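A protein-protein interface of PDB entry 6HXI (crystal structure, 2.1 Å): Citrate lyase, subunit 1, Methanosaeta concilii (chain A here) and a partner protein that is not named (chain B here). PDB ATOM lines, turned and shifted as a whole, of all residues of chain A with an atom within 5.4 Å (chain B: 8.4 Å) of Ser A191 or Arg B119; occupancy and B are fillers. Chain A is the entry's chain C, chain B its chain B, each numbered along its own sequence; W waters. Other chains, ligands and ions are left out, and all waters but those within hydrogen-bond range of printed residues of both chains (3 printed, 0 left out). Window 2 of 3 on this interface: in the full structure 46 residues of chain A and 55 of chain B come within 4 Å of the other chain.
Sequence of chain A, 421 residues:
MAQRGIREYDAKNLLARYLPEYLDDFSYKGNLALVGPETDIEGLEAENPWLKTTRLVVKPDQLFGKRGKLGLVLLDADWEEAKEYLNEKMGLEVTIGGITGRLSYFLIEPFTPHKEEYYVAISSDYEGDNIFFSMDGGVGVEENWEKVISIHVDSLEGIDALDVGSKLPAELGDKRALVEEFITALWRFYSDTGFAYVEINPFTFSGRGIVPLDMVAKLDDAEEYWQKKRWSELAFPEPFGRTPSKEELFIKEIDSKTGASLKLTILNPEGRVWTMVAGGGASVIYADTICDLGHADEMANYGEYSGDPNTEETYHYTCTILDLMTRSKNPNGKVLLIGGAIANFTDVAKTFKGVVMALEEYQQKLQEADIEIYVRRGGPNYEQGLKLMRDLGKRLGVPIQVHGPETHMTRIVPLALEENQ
Of chain B, only Arg B119 comes within 4 Å of Ser A191.
Of chain A, only Asp A129 (3.6 Å), Ser A191 (3.6 Å) and Glu A223 (3.9 Å) come within 4 Å of Arg B119.
Of the printed residues of chain B, Asp A220 touches Pro B117 (3.3 Å) and Glu B118 (2.8 Å).
Of the printed residues of chain B, Ser A155 touches Arg B122 (3.8 Å) and Ala B126 (3.97 Å).
Of the printed residues of chain A, Glu B118 touches Asp A220.
Of the printed residues of chain B, Glu A223 touches Pro B117 (3.7 Å) and Arg B119 (3.9 Å).
Printed residues of chain A within 4 Å of Arg B122: Asp A129 and Ser A155.
The nearest printed residue of chain B that does not touch Ser A191 is Arg B122 (6.8 Å).
The nearest residue of chain A that does not touch Arg B119 is Ser A155 (4.1 Å).
NH2 of Arg B119 lies within salt-bridge range of OD2 of Asp A129 (3.6 Å).
NH1 of Arg B122 lies within salt-bridge range of OD1 of Asp A129, at 3.7 Å.
OD2 of Asp A220 is in hydrogen-bond range of N of Glu B118, at 2.8 Å.
Water W1 lies within hydrogen-bond range of OD2 of Asp A220 (2.7 Å), OE1 of Glu A223 (2.8 Å), N of Arg B119 (2.9 Å) and N of Glu B118 (3.3 Å).
Water W3 lies within hydrogen-bond range of the guanidinium group of Arg B122 (2.8 Å), the guanidinium group of Arg B119 (2.9 Å) and the side-chain carboxylate of Asp A129 (3.0 Å).
Water W2 bridges the backbone carbonyl oxygen of Ser A155 (2.9 Å) and the guanidinium group of Arg B119 (3.2 Å).
Among the printed residues, pairs that only touch across the chains: Asp A220 with Pro B117 (3.3 Å), Ser A191 with Arg B119 (3.6 Å), Glu A223 with Pro B117 (3.7 Å), Ser A155 with Arg B122 (3.8 Å), Glu A223 with Arg B119 (3.9 Å) and Ser A155 with Ala B126 (3.97 Å).
Printed residues of chain A that touch a printed residue of chain B: Asp A129, Ser A155, Ser A191, Asp A220 and Glu A223.
Along chain B the printed residues that touch a printed residue of chain A span positions 117 to 126.
Among the printed residues, 9 pairs touch across the chains.
Among the printed residues, Asp or Glu carboxylates within 4 Å of a Lys or Arg side-chain nitrogen of the other chain: Asp A129 with Arg B119 (3.6 Å) and Asp A129 with Arg B122 (3.7 Å).
NE1 of Trp A187 lies within hydrogen-bond range of OD2 of Asp A129 (2.8 Å).
The side-chain hydroxyl (OG) of Ser A191 sits close to the backbone carbonyl oxygen (O) of Trp A187 (3.5 Å).
The backbone NH (N) of Asp A220 is in hydrogen-bond range of the backbone carbonyl oxygen (O) of Gly A194 (2.9 Å).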
ATOM      1  N   ASP A 129       6.622  11.109 -20.011  1.00  0.00           N
ATOM      2  CA  ASP A 129       5.785  10.419 -19.024  1.00  0.00           C
ATOM      3  C   ASP A 129       4.355  10.916 -19.108  1.00  0.00           C
ATOM      4  O   ASP A 129       4.123  12.092 -19.392  1.00  0.00           O
ATOM      5  CB  ASP A 129       6.338  10.629 -17.605  1.00  0.00           C
ATOM      6  CG  ASP A 129       7.845  10.431 -17.508  1.00  0.00           C
ATOM      7  OD1 ASP A 129       8.352   9.437 -18.077  1.00  0.00           O
ATOM      8  OD2 ASP A 129       8.517  11.277 -16.874  1.00  0.00           O
ATOM      9  N   SER A 155      10.124  14.732 -21.731  1.00  0.00           N
ATOM     10  CA  SER A 155      11.384  14.205 -21.207  1.00  0.00           C
ATOM     11  C   SER A 155      12.391  15.288 -20.833  1.00  0.00           C
ATOM     12  O   SER A 155      13.034  15.195 -19.785  1.00  0.00           O
ATOM     13  CB  SER A 155      12.015  13.219 -22.188  1.00  0.00           C
ATOM     14  OG  SER A 155      11.359  11.963 -22.145  1.00  0.00           O
ATOM     15  N   LEU A 186       4.318  13.148  -6.966  1.00  0.00           N
ATOM     16  CA  LEU A 186       4.291  11.750  -7.400  1.00  0.00           C
ATOM     17  C   LEU A 186       5.122  11.547  -8.657  1.00  0.00           C
ATOM     18  O   LEU A 186       5.819  10.537  -8.747  1.00  0.00           O
ATOM     19  CB  LEU A 186       2.861  11.239  -7.599  1.00  0.00           C
ATOM     20  CG  LEU A 186       2.700   9.715  -7.657  1.00  0.00           C
ATOM     21  CD1 LEU A 186       2.774   9.110  -6.273  1.00  0.00           C
ATOM     22  CD2 LEU A 186       1.388   9.341  -8.316  1.00  0.00           C
ATOM     23  N   TRP A 187       5.084  12.523  -9.599  1.00  0.00           N
ATOM     24  CA  TRP A 187       5.910  12.499 -10.814  1.00  0.00           C
ATOM     25  C   TRP A 187       7.399  12.593 -10.447  1.00  0.00           C
ATOM     26  O   TRP A 187       8.211  11.878 -11.028  1.00  0.00           O
ATOM     27  CB  TRP A 187       5.545  13.624 -11.797  1.00  0.00           C
ATOM     28  CG  TRP A 187       6.416  13.582 -13.018  1.00  0.00           C
ATOM     29  CD1 TRP A 187       6.319  12.710 -14.063  1.00  0.00           C
ATOM     30  CD2 TRP A 187       7.611  14.335 -13.234  1.00  0.00           C
ATOM     31  NE1 TRP A 187       7.354  12.910 -14.945  1.00  0.00           N
ATOM     32  CE2 TRP A 187       8.179  13.884 -14.448  1.00  0.00           C
ATOM     33  CE3 TRP A 187       8.283  15.329 -12.498  1.00  0.00           C
ATOM     34  CZ2 TRP A 187       9.350  14.439 -14.978  1.00  0.00           C
ATOM     35  CZ3 TRP A 187       9.434  15.889 -13.027  1.00  0.00           C
ATOM     36  CH2 TRP A 187       9.961  15.441 -14.252  1.00  0.00           C
ATOM     37  N   ARG A 188       7.747  13.478  -9.494  1.00  0.00           N
ATOM     38  CA  ARG A 188       9.125  13.676  -9.038  1.00  0.00           C
ATOM     39  C   ARG A 188       9.617  12.391  -8.382  1.00  0.00           C
ATOM     40  O   ARG A 188      10.728  11.944  -8.654  1.00  0.00           O
ATOM     41  CB  ARG A 188       9.202  14.874  -8.073  1.00  0.00           C
ATOM     42  CG  ARG A 188       8.834  16.205  -8.714  1.00  0.00           C
ATOM     43  CD  ARG A 188       9.310  17.360  -7.847  1.00  0.00           C
ATOM     44  NE  ARG A 188       8.581  18.603  -8.114  1.00  0.00           N
ATOM     45  CZ  ARG A 188       8.894  19.481  -9.066  1.00  0.00           C
ATOM     46  NH1 ARG A 188       9.909  19.247  -9.893  1.00  0.00           N
ATOM     47  NH2 ARG A 188       8.174  20.582  -9.221  1.00  0.00           N
ATOM     48  N   PHE A 189       8.746  11.761  -7.591  1.00  0.00           N
ATOM     49  CA  PHE A 189       8.984  10.486  -6.943  1.00  0.00           C
ATOM     50  C   PHE A 189       9.191   9.385  -8.001  1.00  0.00           C
ATOM     51  O   PHE A 189      10.120   8.602  -7.887  1.00  0.00           O
ATOM     52  CB  PHE A 189       7.809  10.171  -6.000  1.00  0.00           C
ATOM     53  CG  PHE A 189       7.767   8.785  -5.402  1.00  0.00           C
ATOM     54  CD1 PHE A 189       8.630   8.430  -4.372  1.00  0.00           C
ATOM     55  CD2 PHE A 189       6.835   7.847  -5.844  1.00  0.00           C
ATOM     56  CE1 PHE A 189       8.590   7.150  -3.815  1.00  0.00           C
ATOM     57  CE2 PHE A 189       6.796   6.565  -5.287  1.00  0.00           C
ATOM     58  CZ  PHE A 189       7.677   6.224  -4.273  1.00  0.00           C
ATOM     59  N   TYR A 190       8.359   9.370  -9.045  1.00  0.00           N
ATOM     60  CA  TYR A 190       8.418   8.413 -10.165  1.00  0.00           C
ATOM     61  C   TYR A 190       9.771   8.556 -10.905  1.00  0.00           C
ATOM     62  O   TYR A 190      10.477   7.564 -11.136  1.00  0.00           O
ATOM     63  CB  TYR A 190       7.224   8.702 -11.104  1.00  0.00           C
ATOM     64  CG  TYR A 190       7.182   7.895 -12.386  1.00  0.00           C
ATOM     65  CD1 TYR A 190       6.510   6.680 -12.446  1.00  0.00           C
ATOM     66  CD2 TYR A 190       7.728   8.395 -13.569  1.00  0.00           C
ATOM     67  CE1 TYR A 190       6.446   5.945 -13.630  1.00  0.00           C
ATOM     68  CE2 TYR A 190       7.647   7.682 -14.760  1.00  0.00           C
ATOM     69  CZ  TYR A 190       7.011   6.454 -14.784  1.00  0.00           C
ATOM     70  OH  TYR A 190       6.940   5.736 -15.949  1.00  0.00           O
ATOM     71  N   SER A 191      10.124   9.812 -11.221  1.00  0.00           N
ATOM     72  CA  SER A 191      11.311  10.237 -11.954  1.00  0.00           C
ATOM     73  C   SER A 191      12.633  10.015 -11.242  1.00  0.00           C
ATOM     74  O   SER A 191      13.617   9.680 -11.896  1.00  0.00           O
ATOM     75  CB  SER A 191      11.181  11.705 -12.342  1.00  0.00           C
ATOM     76  OG  SER A 191      10.550  11.780 -13.608  1.00  0.00           O
ATOM     77  N   ASP A 192      12.680  10.255  -9.928  1.00  0.00           N
ATOM     78  CA  ASP A 192      13.912  10.121  -9.159  1.00  0.00           C
ATOM     79  C   ASP A 192      14.130   8.743  -8.548  1.00  0.00           C
ATOM     80  O   ASP A 192      15.284   8.421  -8.221  1.00  0.00           O
ATOM     81  CB  ASP A 192      13.994  11.209  -8.075  1.00  0.00           C
ATOM     82  CG  ASP A 192      13.937  12.653  -8.563  1.00  0.00           C
ATOM     83  OD1 ASP A 192      14.248  12.895  -9.756  1.00  0.00           O
ATOM     84  OD2 ASP A 192      13.616  13.544  -7.740  1.00  0.00           O
ATOM     85  N   THR A 193      13.057   7.921  -8.416  1.00  0.00           N
ATOM     86  CA  THR A 193      13.152   6.597  -7.790  1.00  0.00           C
ATOM     87  C   THR A 193      13.164   5.422  -8.819  1.00  0.00           C
ATOM     88  O   THR A 193      13.157   4.257  -8.413  1.00  0.00           O
ATOM     89  CB  THR A 193      12.083   6.448  -6.699  1.00  0.00           C
ATOM     90  OG1 THR A 193      11.903   7.719  -6.091  1.00  0.00           O
ATOM     91  CG2 THR A 193      12.476   5.453  -5.605  1.00  0.00           C
ATOM     92  N   GLY A 194      13.261   5.734 -10.109  1.00  0.00           N
ATOM     93  CA  GLY A 194      13.404   4.733 -11.164  1.00  0.00           C
ATOM     94  C   GLY A 194      12.232   3.813 -11.430  1.00  0.00           C
ATOM     95  O   GLY A 194      12.418   2.632 -11.726  1.00  0.00           O
ATOM     96  N   ASP A 220      12.117   0.045 -13.086  1.00  0.00           N
ATOM     97  CA  ASP A 220      12.994  -0.285 -14.200  1.00  0.00           C
ATOM     98  C   ASP A 220      14.242  -0.854 -13.511  1.00  0.00           C
ATOM     99  O   ASP A 220      14.976  -0.087 -12.867  1.00  0.00           O
ATOM    100  CB  ASP A 220      13.346   0.970 -15.005  1.00  0.00           C
ATOM    101  CG  ASP A 220      14.491   0.785 -15.995  1.00  0.00           C
ATOM    102  OD1 ASP A 220      14.737  -0.370 -16.423  1.00  0.00           O
ATOM    103  OD2 ASP A 220      15.125   1.792 -16.357  1.00  0.00           O
ATOM    104  N   GLU A 223      17.878   0.662 -13.268  1.00  0.00           N
ATOM    105  CA  GLU A 223      18.083   1.810 -12.365  1.00  0.00           C
ATOM    106  C   GLU A 223      18.848   1.465 -11.076  1.00  0.00           C
ATOM    107  O   GLU A 223      19.292   2.383 -10.376  1.00  0.00           O
ATOM    108  CB  GLU A 223      16.719   2.437 -11.996  1.00  0.00           C
ATOM    109  CG  GLU A 223      16.077   3.219 -13.122  1.00  0.00           C
ATOM    110  CD  GLU A 223      16.357   4.708 -13.141  1.00  0.00           C
ATOM    111  OE1 GLU A 223      15.742   5.405 -13.980  1.00  0.00           O
ATOM    112  OE2 GLU A 223      17.159   5.186 -12.306  1.00  0.00           O
ATOM    113  N   PHE B  94      25.080   7.355 -20.521  1.00  0.00           N
ATOM    114  CA  PHE B  94      24.307   8.595 -20.571  1.00  0.00           C
ATOM    115  C   PHE B  94      25.165   9.849 -20.613  1.00  0.00           C
ATOM    116  O   PHE B  94      25.029  10.640 -21.539  1.00  0.00           O
ATOM    117  CB  PHE B  94      23.287   8.667 -19.429  1.00  0.00           C
ATOM    118  CG  PHE B  94      22.386   9.886 -19.427  1.00  0.00           C
ATOM    119  CD1 PHE B  94      21.279   9.957 -20.264  1.00  0.00           C
ATOM    120  CD2 PHE B  94      22.613  10.938 -18.541  1.00  0.00           C
ATOM    121  CE1 PHE B  94      20.443  11.080 -20.247  1.00  0.00           C
ATOM    122  CE2 PHE B  94      21.772  12.053 -18.519  1.00  0.00           C
ATOM    123  CZ  PHE B  94      20.691  12.115 -19.368  1.00  0.00           C
ATOM    124  N   VAL B 116      21.118   0.201 -19.757  1.00  0.00           N
ATOM    125  CA  VAL B 116      20.953   1.647 -19.595  1.00  0.00           C
ATOM    126  C   VAL B 116      19.508   1.927 -19.128  1.00  0.00           C
ATOM    127  O   VAL B 116      18.569   1.430 -19.755  1.00  0.00           O
ATOM    128  CB  VAL B 116      21.314   2.439 -20.893  1.00  0.00           C
ATOM    129  CG1 VAL B 116      21.082   3.943 -20.727  1.00  0.00           C
ATOM    130  CG2 VAL B 116      22.756   2.169 -21.331  1.00  0.00           C
ATOM    131  N   PRO B 117      19.295   2.727 -18.051  1.00  0.00           N
ATOM    132  CA  PRO B 117      17.911   3.031 -17.620  1.00  0.00           C
ATOM    133  C   PRO B 117      17.038   3.556 -18.732  1.00  0.00           C
ATOM    134  O   PRO B 117      17.506   4.289 -19.600  1.00  0.00           O
ATOM    135  CB  PRO B 117      18.094   4.096 -16.531  1.00  0.00           C
ATOM    136  CG  PRO B 117      19.431   3.814 -15.987  1.00  0.00           C
ATOM    137  CD  PRO B 117      20.277   3.386 -17.171  1.00  0.00           C
ATOM    138  N   GLU B 118      15.753   3.175 -18.703  1.00  0.00           N
ATOM    139  CA  GLU B 118      14.754   3.595 -19.695  1.00  0.00           C
ATOM    140  C   GLU B 118      14.592   5.113 -19.703  1.00  0.00           C
ATOM    141  O   GLU B 118      14.504   5.699 -20.785  1.00  0.00           O
ATOM    142  CB  GLU B 118      13.436   2.871 -19.460  1.00  0.00           C
ATOM    143  CG  GLU B 118      13.514   1.399 -19.823  1.00  0.00           C
ATOM    144  CD  GLU B 118      12.422   0.464 -19.331  1.00  0.00           C
ATOM    145  OE1 GLU B 118      11.373   0.951 -18.855  1.00  0.00           O
ATOM    146  OE2 GLU B 118      12.613  -0.767 -19.449  1.00  0.00           O
ATOM    147  N   ARG B 119      14.644   5.751 -18.504  1.00  0.00           N
ATOM    148  CA  ARG B 119      14.550   7.209 -18.384  1.00  0.00           C
ATOM    149  C   ARG B 119      15.704   7.955 -19.112  1.00  0.00           C
ATOM    150  O   ARG B 119      15.447   8.924 -19.824  1.00  0.00           O
ATOM    151  CB  ARG B 119      14.408   7.662 -16.925  1.00  0.00           C
ATOM    152  CG  ARG B 119      14.449   9.180 -16.796  1.00  0.00           C
ATOM    153  CD  ARG B 119      13.887   9.757 -15.523  1.00  0.00           C
ATOM    154  NE  ARG B 119      14.009  11.214 -15.572  1.00  0.00           N
ATOM    155  CZ  ARG B 119      13.157  12.029 -16.194  1.00  0.00           C
ATOM    156  NH1 ARG B 119      13.371  13.339 -16.201  1.00  0.00           N
ATOM    157  NH2 ARG B 119      12.080  11.539 -16.808  1.00  0.00           N
ATOM    158  N   GLN B 120      16.945   7.477 -18.942  1.00  0.00           N
ATOM    159  CA  GLN B 120      18.160   7.983 -19.577  1.00  0.00           C
ATOM    160  C   GLN B 120      18.069   7.866 -21.105  1.00  0.00           C
ATOM    161  O   GLN B 120      18.387   8.832 -21.806  1.00  0.00           O
ATOM    162  CB  GLN B 120      19.386   7.227 -19.060  1.00  0.00           C
ATOM    163  CG  GLN B 120      19.790   7.630 -17.628  1.00  0.00           C
ATOM    164  CD  GLN B 120      20.994   6.872 -17.119  1.00  0.00           C
ATOM    165  OE1 GLN B 120      21.810   6.349 -17.882  1.00  0.00           O
ATOM    166  NE2 GLN B 120      21.118   6.758 -15.810  1.00  0.00           N
ATOM    167  N   SER B 121      17.584   6.707 -21.613  1.00  0.00           N
ATOM    168  CA  SER B 121      17.403   6.479 -23.060  1.00  0.00           C
ATOM    169  C   SER B 121      16.367   7.437 -23.642  1.00  0.00           C
ATOM    170  O   SER B 121      16.600   7.982 -24.721  1.00  0.00           O
ATOM    171  CB  SER B 121      17.024   5.038 -23.335  1.00  0.00           C
ATOM    172  OG  SER B 121      18.161   4.252 -23.047  1.00  0.00           O
ATOM    173  N   ARG B 122      15.240   7.656 -22.933  1.00  0.00           N
ATOM    174  CA  ARG B 122      14.204   8.605 -23.354  1.00  0.00           C
ATOM    175  C   ARG B 122      14.785  10.029 -23.423  1.00  0.00           C
ATOM    176  O   ARG B 122      14.513  10.756 -24.375  1.00  0.00           O
ATOM    177  CB  ARG B 122      13.024   8.597 -22.380  1.00  0.00           C
ATOM    178  CG  ARG B 122      12.116   7.403 -22.499  1.00  0.00           C
ATOM    179  CD  ARG B 122      10.787   7.654 -21.806  1.00  0.00           C
ATOM    180  NE  ARG B 122      10.911   7.712 -20.346  1.00  0.00           N
ATOM    181  CZ  ARG B 122      10.891   6.645 -19.549  1.00  0.00           C
ATOM    182  NH1 ARG B 122      10.996   6.791 -18.235  1.00  0.00           N
ATOM    183  NH2 ARG B 122      10.726   5.429 -20.058  1.00  0.00           N
ATOM    184  N   VAL B 123      15.606  10.414 -22.429  1.00  0.00           N
ATOM    185  CA  VAL B 123      16.262  11.743 -22.403  1.00  0.00           C
ATOM    186  C   VAL B 123      17.285  11.868 -23.560  1.00  0.00           C
ATOM    187  O   VAL B 123      17.362  12.933 -24.162  1.00  0.00           O
ATOM    188  CB  VAL B 123      16.851  12.119 -21.023  1.00  0.00           C
ATOM    189  CG1 VAL B 123      17.679  13.405 -21.105  1.00  0.00           C
ATOM    190  CG2 VAL B 123      15.739  12.251 -19.979  1.00  0.00           C
ATOM    191  N   MET B 124      17.999  10.774 -23.908  1.00  0.00           N
ATOM    192  CA  MET B 124      18.952  10.781 -25.026  1.00  0.00           C
ATOM    193  C   MET B 124      18.220  10.921 -26.364  1.00  0.00           C
ATOM    194  O   MET B 124      18.625  11.737 -27.191  1.00  0.00           O
ATOM    195  CB  MET B 124      19.844   9.528 -25.016  1.00  0.00           C
ATOM    196  CG  MET B 124      20.819   9.522 -23.862  1.00  0.00           C
ATOM    197  SD  MET B 124      22.068   8.222 -23.911  1.00  0.00           S
ATOM    198  CE  MET B 124      21.111   6.796 -23.505  1.00  0.00           C
ATOM    199  N   ALA B 125      17.128  10.137 -26.551  1.00  0.00           N
ATOM    200  CA  ALA B 125      16.263  10.135 -27.733  1.00  0.00           C
ATOM    201  C   ALA B 125      15.676  11.498 -27.974  1.00  0.00           C
ATOM    202  O   ALA B 125      15.761  11.982 -29.100  1.00  0.00           O
ATOM    203  CB  ALA B 125      15.144   9.105 -27.584  1.00  0.00           C
ATOM    204  N   ALA B 126      15.103  12.136 -26.916  1.00  0.00           N
ATOM    205  CA  ALA B 126      14.512  13.469 -26.987  1.00  0.00           C
ATOM    206  C   ALA B 126      15.597  14.533 -27.296  1.00  0.00           C
ATOM    207  O   ALA B 126      15.352  15.426 -28.113  1.00  0.00           O
ATOM    208  CB  ALA B 126      13.815  13.790 -25.684  1.00  0.00           C
ATOM    209  N   TYR B 207      12.758   1.791 -24.837  1.00  0.00           N
ATOM    210  CA  TYR B 207      12.813   3.184 -25.278  1.00  0.00           C
ATOM    211  C   TYR B 207      14.112   3.415 -26.021  1.00  0.00           C
ATOM    212  O   TYR B 207      15.119   3.734 -25.393  1.00  0.00           O
ATOM    213  CB  TYR B 207      12.637   4.139 -24.077  1.00  0.00           C
ATOM    214  CG  TYR B 207      11.324   3.915 -23.363  1.00  0.00           C
ATOM    215  CD1 TYR B 207      10.153   4.537 -23.798  1.00  0.00           C
ATOM    216  CD2 TYR B 207      11.231   3.022 -22.295  1.00  0.00           C
ATOM    217  CE1 TYR B 207       8.925   4.291 -23.176  1.00  0.00           C
ATOM    218  CE2 TYR B 207      10.009   2.768 -21.667  1.00  0.00           C
ATOM    219  CZ  TYR B 207       8.862   3.408 -22.111  1.00  0.00           C
ATOM    220  OH  TYR B 207       7.665   3.144 -21.504  1.00  0.00           O
HETATM  221  O   HOH W   1      14.139   4.293 -16.034  1.00  0.00           O
HETATM  222  O   HOH W   2      11.067  15.054 -17.648  1.00  0.00           O
HETATM  223  O   HOH W   3      10.846   8.914 -16.461  1.00  0.00           O
